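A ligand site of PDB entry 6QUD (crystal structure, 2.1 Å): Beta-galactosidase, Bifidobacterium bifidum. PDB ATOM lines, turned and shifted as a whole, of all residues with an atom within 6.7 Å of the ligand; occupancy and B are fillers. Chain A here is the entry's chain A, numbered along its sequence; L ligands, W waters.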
ATOM      1  N   ARG A 165      -3.166  -7.820 -14.607  1.00  0.00           N
ATOM      2  CA  ARG A 165      -2.317  -6.814 -13.979  1.00  0.00           C
ATOM      3  C   ARG A 165      -0.981  -7.380 -13.509  1.00  0.00           C
ATOM      4  O   ARG A 165      -0.124  -6.599 -13.072  1.00  0.00           O
ATOM      5  CB  ARG A 165      -3.048  -6.189 -12.785  1.00  0.00           C
ATOM      6  CG  ARG A 165      -4.439  -5.676 -13.116  1.00  0.00           C
ATOM      7  CD  ARG A 165      -5.098  -4.971 -11.918  1.00  0.00           C
ATOM      8  NE  ARG A 165      -5.354  -5.881 -10.808  1.00  0.00           N
ATOM      9  CZ  ARG A 165      -4.603  -5.944  -9.712  1.00  0.00           C
ATOM     10  NH1 ARG A 165      -3.535  -5.162  -9.579  1.00  0.00           N
ATOM     11  NH2 ARG A 165      -4.907  -6.792  -8.741  1.00  0.00           N
ATOM     12  N   TRP A 166      -0.790  -8.689 -13.585  1.00  0.00           N
ATOM     13  CA  TRP A 166       0.474  -9.327 -13.241  1.00  0.00           C
ATOM     14  C   TRP A 166       0.759 -10.428 -14.252  1.00  0.00           C
ATOM     15  O   TRP A 166      -0.081 -10.758 -15.093  1.00  0.00           O
ATOM     16  CB  TRP A 166       0.437  -9.888 -11.812  1.00  0.00           C
ATOM     17  CG  TRP A 166      -0.623 -10.935 -11.624  1.00  0.00           C
ATOM     18  CD1 TRP A 166      -0.478 -12.283 -11.806  1.00  0.00           C
ATOM     19  CD2 TRP A 166      -1.981 -10.722 -11.218  1.00  0.00           C
ATOM     20  NE1 TRP A 166      -1.663 -12.918 -11.538  1.00  0.00           N
ATOM     21  CE2 TRP A 166      -2.607 -11.983 -11.175  1.00  0.00           C
ATOM     22  CE3 TRP A 166      -2.729  -9.587 -10.876  1.00  0.00           C
ATOM     23  CZ2 TRP A 166      -3.943 -12.148 -10.806  1.00  0.00           C
ATOM     24  CZ3 TRP A 166      -4.058  -9.748 -10.519  1.00  0.00           C
ATOM     25  CH2 TRP A 166      -4.646 -11.017 -10.489  1.00  0.00           C
ATOM     26  N   HIS A 327       1.860 -14.009  -5.005  1.00  0.00           N
ATOM     27  CA  HIS A 327       1.437 -14.424  -6.322  1.00  0.00           C
ATOM     28  C   HIS A 327       1.921 -15.849  -6.595  1.00  0.00           C
ATOM     29  O   HIS A 327       2.706 -16.421  -5.822  1.00  0.00           O
ATOM     30  CB  HIS A 327       1.940 -13.466  -7.388  1.00  0.00           C
ATOM     31  CG  HIS A 327       1.012 -12.322  -7.657  1.00  0.00           C
ATOM     32  ND1 HIS A 327      -0.259 -12.490  -8.152  1.00  0.00           N
ATOM     33  CD2 HIS A 327       1.176 -10.983  -7.485  1.00  0.00           C
ATOM     34  CE1 HIS A 327      -0.840 -11.315  -8.277  1.00  0.00           C
ATOM     35  NE2 HIS A 327       0.012 -10.385  -7.885  1.00  0.00           N
ATOM     36  N   ARG A 358      -1.713 -15.150   1.936  1.00  0.00           N
ATOM     37  CA  ARG A 358      -2.910 -14.773   1.188  1.00  0.00           C
ATOM     38  C   ARG A 358      -2.636 -15.003  -0.293  1.00  0.00           C
ATOM     39  O   ARG A 358      -1.701 -14.411  -0.850  1.00  0.00           O
ATOM     40  CB  ARG A 358      -3.292 -13.313   1.461  1.00  0.00           C
ATOM     41  CG  ARG A 358      -4.633 -12.884   0.877  1.00  0.00           C
ATOM     42  CD  ARG A 358      -4.789 -11.371   0.953  1.00  0.00           C
ATOM     43  NE  ARG A 358      -6.012 -10.904   0.309  1.00  0.00           N
ATOM     44  CZ  ARG A 358      -6.163  -9.718  -0.266  1.00  0.00           C
ATOM     45  NH1 ARG A 358      -5.145  -8.861  -0.278  1.00  0.00           N
ATOM     46  NH2 ARG A 358      -7.313  -9.374  -0.838  1.00  0.00           N
ATOM     47  N   THR A 360      -3.099 -14.102  -3.374  1.00  0.00           N
ATOM     48  CA  THR A 360      -3.548 -12.995  -4.194  1.00  0.00           C
ATOM     49  C   THR A 360      -3.240 -13.254  -5.664  1.00  0.00           C
ATOM     50  O   THR A 360      -2.102 -13.571  -6.011  1.00  0.00           O
ATOM     51  CB  THR A 360      -2.867 -11.706  -3.745  1.00  0.00           C
ATOM     52  OG1 THR A 360      -1.441 -11.884  -3.805  1.00  0.00           O
ATOM     53  CG2 THR A 360      -3.264 -11.341  -2.329  1.00  0.00           C
ATOM     54  N   HIS A 361      -4.246 -13.123  -6.537  1.00  0.00           N
ATOM     55  CA  HIS A 361      -5.654 -12.955  -6.171  1.00  0.00           C
ATOM     56  C   HIS A 361      -6.443 -14.060  -6.859  1.00  0.00           C
ATOM     57  O   HIS A 361      -7.275 -13.782  -7.727  1.00  0.00           O
ATOM     58  CB  HIS A 361      -6.202 -11.590  -6.627  1.00  0.00           C
ATOM     59  CG  HIS A 361      -5.491 -10.417  -6.034  1.00  0.00           C
ATOM     60  ND1 HIS A 361      -5.648 -10.026  -4.728  1.00  0.00           N
ATOM     61  CD2 HIS A 361      -4.636  -9.516  -6.590  1.00  0.00           C
ATOM     62  CE1 HIS A 361      -4.922  -8.948  -4.485  1.00  0.00           C
ATOM     63  NE2 HIS A 361      -4.303  -8.615  -5.610  1.00  0.00           N
ATOM     64  N   ASP A 385     -10.029 -11.722  -8.325  1.00  0.00           N
ATOM     65  CA  ASP A 385      -9.477 -10.380  -8.211  1.00  0.00           C
ATOM     66  C   ASP A 385     -10.629  -9.387  -8.205  1.00  0.00           C
ATOM     67  O   ASP A 385     -11.090  -8.954  -7.147  1.00  0.00           O
ATOM     68  CB  ASP A 385      -8.500 -10.092  -9.352  1.00  0.00           C
ATOM     69  CG  ASP A 385      -7.746  -8.769  -9.178  1.00  0.00           C
ATOM     70  OD1 ASP A 385      -7.681  -8.262  -8.038  1.00  0.00           O
ATOM     71  OD2 ASP A 385      -7.225  -8.251 -10.183  1.00  0.00           O
ATOM     72  N   ASN A 446     -10.793  -8.494  -4.403  1.00  0.00           N
ATOM     73  CA  ASN A 446      -9.966  -7.359  -4.004  1.00  0.00           C
ATOM     74  C   ASN A 446     -10.397  -6.156  -4.822  1.00  0.00           C
ATOM     75  O   ASN A 446     -10.334  -6.180  -6.054  1.00  0.00           O
ATOM     76  CB  ASN A 446      -8.481  -7.660  -4.247  1.00  0.00           C
ATOM     77  CG  ASN A 446      -7.568  -6.643  -3.609  1.00  0.00           C
ATOM     78  OD1 ASN A 446      -7.124  -6.806  -2.473  1.00  0.00           O
ATOM     79  ND2 ASN A 446      -7.271  -5.567  -4.342  1.00  0.00           N
ATOM     80  N   ASN A 510      -7.597  -2.636   2.911  1.00  0.00           N
ATOM     81  CA  ASN A 510      -6.360  -2.550   2.151  1.00  0.00           C
ATOM     82  C   ASN A 510      -5.714  -1.183   2.396  1.00  0.00           C
ATOM     83  O   ASN A 510      -6.344  -0.153   2.187  1.00  0.00           O
ATOM     84  CB  ASN A 510      -6.618  -2.743   0.661  1.00  0.00           C
ATOM     85  CG  ASN A 510      -6.999  -4.176   0.315  1.00  0.00           C
ATOM     86  OD1 ASN A 510      -6.883  -5.077   1.148  1.00  0.00           O
ATOM     87  ND2 ASN A 510      -7.457  -4.387  -0.914  1.00  0.00           N
ATOM     88  N   TYR A 511      -4.457  -1.205   2.856  1.00  0.00           N
ATOM     89  CA  TYR A 511      -3.625  -0.014   2.963  1.00  0.00           C
ATOM     90  C   TYR A 511      -4.224   1.021   3.907  1.00  0.00           C
ATOM     91  O   TYR A 511      -4.217   2.225   3.624  1.00  0.00           O
ATOM     92  CB  TYR A 511      -3.346   0.592   1.589  1.00  0.00           C
ATOM     93  CG  TYR A 511      -2.618  -0.355   0.671  1.00  0.00           C
ATOM     94  CD1 TYR A 511      -1.296  -0.705   0.912  1.00  0.00           C
ATOM     95  CD2 TYR A 511      -3.245  -0.903  -0.447  1.00  0.00           C
ATOM     96  CE1 TYR A 511      -0.618  -1.578   0.086  1.00  0.00           C
ATOM     97  CE2 TYR A 511      -2.571  -1.781  -1.286  1.00  0.00           C
ATOM     98  CZ  TYR A 511      -1.260  -2.111  -1.010  1.00  0.00           C
ATOM     99  OH  TYR A 511      -0.585  -2.980  -1.845  1.00  0.00           O
ATOM    100  N   GLU A 533      -4.108  -6.179   2.883  1.00  0.00           N
ATOM    101  CA  GLU A 533      -3.040  -5.849   1.938  1.00  0.00           C
ATOM    102  C   GLU A 533      -2.347  -4.605   2.466  1.00  0.00           C
ATOM    103  O   GLU A 533      -2.974  -3.546   2.550  1.00  0.00           O
ATOM    104  CB  GLU A 533      -3.597  -5.630   0.531  1.00  0.00           C
ATOM    105  CG  GLU A 533      -2.546  -5.338  -0.526  1.00  0.00           C
ATOM    106  CD  GLU A 533      -3.149  -5.155  -1.914  1.00  0.00           C
ATOM    107  OE1 GLU A 533      -4.303  -5.590  -2.107  1.00  0.00           O
ATOM    108  OE2 GLU A 533      -2.483  -4.570  -2.794  1.00  0.00           O
ATOM    109  N   ALA A 535       1.619  -2.317   3.374  1.00  0.00           N
ATOM    110  CA  ALA A 535       2.989  -1.930   3.038  1.00  0.00           C
ATOM    111  C   ALA A 535       3.135  -1.514   1.572  1.00  0.00           C
ATOM    112  O   ALA A 535       2.998  -0.336   1.249  1.00  0.00           O
ATOM    113  CB  ALA A 535       3.974  -3.050   3.370  1.00  0.00           C
ATOM    114  N   SER A 536       3.400  -2.487   0.701  1.00  0.00           N
ATOM    115  CA  SER A 536       3.784  -2.206  -0.698  1.00  0.00           C
ATOM    116  C   SER A 536       5.019  -1.319  -0.745  1.00  0.00           C
ATOM    117  O   SER A 536       5.099  -0.377  -1.534  1.00  0.00           O
ATOM    118  CB  SER A 536       2.633  -1.578  -1.483  1.00  0.00           C
ATOM    119  OG  SER A 536       1.960  -2.544  -2.265  1.00  0.00           O
ATOM    120  N   VAL A 566       5.207   2.918  -2.445  1.00  0.00           N
ATOM    121  CA  VAL A 566       4.297   3.575  -3.373  1.00  0.00           C
ATOM    122  C   VAL A 566       3.448   4.597  -2.637  1.00  0.00           C
ATOM    123  O   VAL A 566       3.280   4.557  -1.415  1.00  0.00           O
ATOM    124  CB  VAL A 566       3.414   2.536  -4.096  1.00  0.00           C
ATOM    125  CG1 VAL A 566       4.280   1.604  -4.921  1.00  0.00           C
ATOM    126  CG2 VAL A 566       2.582   1.768  -3.083  1.00  0.00           C
ATOM    127  N   TRP A 568       0.310   5.135  -2.325  1.00  0.00           N
ATOM    128  CA  TRP A 568      -0.846   4.644  -1.575  1.00  0.00           C
ATOM    129  C   TRP A 568      -0.453   3.656  -0.483  1.00  0.00           C
ATOM    130  O   TRP A 568      -1.345   3.193   0.253  1.00  0.00           O
ATOM    131  CB  TRP A 568      -1.859   3.991  -2.521  1.00  0.00           C
ATOM    132  CG  TRP A 568      -1.317   2.812  -3.265  1.00  0.00           C
ATOM    133  CD1 TRP A 568      -1.381   1.499  -2.891  1.00  0.00           C
ATOM    134  CD2 TRP A 568      -0.631   2.836  -4.521  1.00  0.00           C
ATOM    135  NE1 TRP A 568      -0.776   0.711  -3.829  1.00  0.00           N
ATOM    136  CE2 TRP A 568      -0.308   1.500  -4.847  1.00  0.00           C
ATOM    137  CE3 TRP A 568      -0.258   3.848  -5.405  1.00  0.00           C
ATOM    138  CZ2 TRP A 568       0.370   1.161  -6.013  1.00  0.00           C
ATOM    139  CZ3 TRP A 568       0.421   3.517  -6.567  1.00  0.00           C
ATOM    140  CH2 TRP A 568       0.734   2.179  -6.857  1.00  0.00           C
ATOM    141  N   TRP A 591       2.225  -6.905   1.047  1.00  0.00           N
ATOM    142  CA  TRP A 591       2.378  -6.985  -0.403  1.00  0.00           C
ATOM    143  C   TRP A 591       3.805  -6.574  -0.756  1.00  0.00           C
ATOM    144  O   TRP A 591       4.152  -5.397  -0.648  1.00  0.00           O
ATOM    145  CB  TRP A 591       1.359  -6.073  -1.088  1.00  0.00           C
ATOM    146  CG  TRP A 591       1.362  -6.238  -2.568  1.00  0.00           C
ATOM    147  CD1 TRP A 591       2.154  -5.599  -3.470  1.00  0.00           C
ATOM    148  CD2 TRP A 591       0.530  -7.128  -3.319  1.00  0.00           C
ATOM    149  NE1 TRP A 591       1.878  -6.047  -4.740  1.00  0.00           N
ATOM    150  CE2 TRP A 591       0.886  -6.981  -4.678  1.00  0.00           C
ATOM    151  CE3 TRP A 591      -0.463  -8.047  -2.980  1.00  0.00           C
ATOM    152  CZ2 TRP A 591       0.273  -7.728  -5.685  1.00  0.00           C
ATOM    153  CZ3 TRP A 591      -1.065  -8.776  -3.981  1.00  0.00           C
ATOM    154  CH2 TRP A 591      -0.704  -8.604  -5.321  1.00  0.00           C
ATOM    155  N   TYR A 596       7.484 -10.915  -7.861  1.00  0.00           N
ATOM    156  CA  TYR A 596       6.779 -11.688  -8.865  1.00  0.00           C
ATOM    157  C   TYR A 596       6.967 -11.027 -10.224  1.00  0.00           C
ATOM    158  O   TYR A 596       7.311  -9.849 -10.328  1.00  0.00           O
ATOM    159  CB  TYR A 596       5.277 -11.813  -8.535  1.00  0.00           C
ATOM    160  CG  TYR A 596       4.575 -10.489  -8.314  1.00  0.00           C
ATOM    161  CD1 TYR A 596       4.675  -9.819  -7.101  1.00  0.00           C
ATOM    162  CD2 TYR A 596       3.831  -9.898  -9.326  1.00  0.00           C
ATOM    163  CE1 TYR A 596       4.044  -8.615  -6.896  1.00  0.00           C
ATOM    164  CE2 TYR A 596       3.189  -8.680  -9.124  1.00  0.00           C
ATOM    165  CZ  TYR A 596       3.302  -8.046  -7.907  1.00  0.00           C
ATOM    166  OH  TYR A 596       2.671  -6.841  -7.702  1.00  0.00           O
ATOM    167  N   GLU A 599       3.951  -6.349 -13.033  1.00  0.00           N
ATOM    168  CA  GLU A 599       3.685  -5.156 -12.222  1.00  0.00           C
ATOM    169  C   GLU A 599       4.956  -4.509 -11.675  1.00  0.00           C
ATOM    170  O   GLU A 599       5.158  -4.480 -10.457  1.00  0.00           O
ATOM    171  CB  GLU A 599       2.733  -5.496 -11.066  1.00  0.00           C
ATOM    172  CG  GLU A 599       2.024  -4.279 -10.485  1.00  0.00           C
ATOM    173  CD  GLU A 599       0.970  -4.647  -9.450  1.00  0.00           C
ATOM    174  OE1 GLU A 599       0.952  -5.812  -9.000  1.00  0.00           O
ATOM    175  OE2 GLU A 599       0.161  -3.765  -9.090  1.00  0.00           O
ATOM    176  N   THR A 601       5.987  -1.658 -10.870  1.00  0.00           N
ATOM    177  CA  THR A 601       5.874  -0.343 -10.250  1.00  0.00           C
ATOM    178  C   THR A 601       7.153  -0.033  -9.471  1.00  0.00           C
ATOM    179  O   THR A 601       7.640  -0.896  -8.722  1.00  0.00           O
ATOM    180  CB  THR A 601       4.659  -0.329  -9.318  1.00  0.00           C
ATOM    181  OG1 THR A 601       3.524  -0.874 -10.004  1.00  0.00           O
ATOM    182  CG2 THR A 601       4.330   1.086  -8.843  1.00  0.00           C
ATOM    183  N   PHE A 622       7.976  -5.145  -4.963  1.00  0.00           N
ATOM    184  CA  PHE A 622       7.250  -5.188  -3.704  1.00  0.00           C
ATOM    185  C   PHE A 622       7.760  -6.273  -2.766  1.00  0.00           C
ATOM    186  O   PHE A 622       7.537  -6.167  -1.545  1.00  0.00           O
ATOM    187  CB  PHE A 622       5.757  -5.432  -3.947  1.00  0.00           C
ATOM    188  CG  PHE A 622       5.104  -4.418  -4.843  1.00  0.00           C
ATOM    189  CD1 PHE A 622       4.969  -3.102  -4.430  1.00  0.00           C
ATOM    190  CD2 PHE A 622       4.588  -4.797  -6.074  1.00  0.00           C
ATOM    191  CE1 PHE A 622       4.342  -2.171  -5.235  1.00  0.00           C
ATOM    192  CE2 PHE A 622       3.969  -3.862  -6.891  1.00  0.00           C
ATOM    193  CZ  PHE A 622       3.845  -2.558  -6.475  1.00  0.00           C
HETATM  194  C1  LIG L   1      -3.109  -4.098  -3.959  1.00  0.00           C
HETATM  195  C2  LIG L   1      -3.600  -4.960  -5.105  1.00  0.00           C
HETATM  196  C3  LIG L   1      -2.467  -5.699  -5.715  1.00  0.00           C
HETATM  197  C4  LIG L   1      -1.346  -4.790  -6.160  1.00  0.00           C
HETATM  198  C5  LIG L   1      -0.935  -3.800  -5.071  1.00  0.00           C
HETATM  199  C6  LIG L   1      -0.008  -2.753  -5.650  1.00  0.00           C
HETATM  200  O1  LIG L   1      -2.947  -6.479  -6.851  1.00  0.00           O
HETATM  201  O2  LIG L   1      -1.725  -4.089  -7.347  1.00  0.00           O
HETATM  202  O3  LIG L   1      -2.072  -3.122  -4.442  1.00  0.00           O
HETATM  203  O4  LIG L   1       0.416  -1.909  -4.606  1.00  0.00           O
HETATM  204  O   HOH W   1      -0.845  -7.724  -8.678  1.00  0.00           O
HETATM  205  O   HOH W   2      -1.585  -3.330 -10.755  1.00  0.00           O
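Water W1 lies within hydrogen-bond range of OE1 of Glu 599, NE2 of His 327 and O1 of the ligand.
Water W2 lies within hydrogen-bond range of OE2 of Glu 599 (2.5 Å), NH1 of Arg 165 (2.9 Å) and O2 of the ligand (3.5 Å).
OG of Ser 536 sits at hydrogen-bond distance from OH of Tyr 511, 2.6 Å away.
The side-chain amide oxygen of Asn 446 is in hydrogen-bond range of the guanidinium group of Arg 358.
OE1 of Glu 533 lies close to OD1 of Asn 446 (3.1 Å).
The side-chain carboxylate of Glu 599 is in salt-bridge range of the guanidinium group of Arg 165 (3.98 Å).
The side-chain amide oxygen (OD1) of Asn 446 is in hydrogen-bond range of the side-chain amide nitrogen (ND2) of Asn 510.
The backbone NH of Val 566 is in hydrogen-bond range of the backbone carbonyl oxygen of Ser 536 (3.4 Å).
OE1 of Glu 533 lies within salt-bridge range of NH1 of Arg 358 (3.8 Å).
The backbone NH of Glu 533 lies close to the side-chain amide oxygen of Asn 510.
Asn 446 touches the ligand.
Trp 591 touches the ligand.
Phe 622 touches the ligand.
Hydrophobic or aromatic side chains that line the ligand: His 361, Tyr 511, Trp 568, Trp 591 and Phe 622.
The nearest printed residue that does not touch the ligand is Val 566 (4.5 Å).
An oxygen (O4) of the ligand lies within hydrogen-bond range of the indole nitrogen of Trp 568 (3.0 Å).
An oxygen (O4) of the ligand lies within hydrogen-bond range of the side-chain hydroxyl (OG) of Ser 536.
The side-chain carboxylate (OE2) of Glu 533 is bonded to a carbon (C1) of the ligand, 1.4 Å away.
The side-chain carboxylate (OE2) of Glu 599 sits at hydrogen-bond distance from an oxygen (O2) of the ligand (2.6 Å).
O1 of the ligand sits at hydrogen-bond distance from NH2 of Arg 165 (2.7 Å).
An oxygen (O3) of the ligand lies within hydrogen-bond range of the side-chain hydroxyl of Tyr 511 (3.0 Å).
NE2 of His 361 lies within hydrogen-bond range of O1 of the ligand (2.8 Å).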
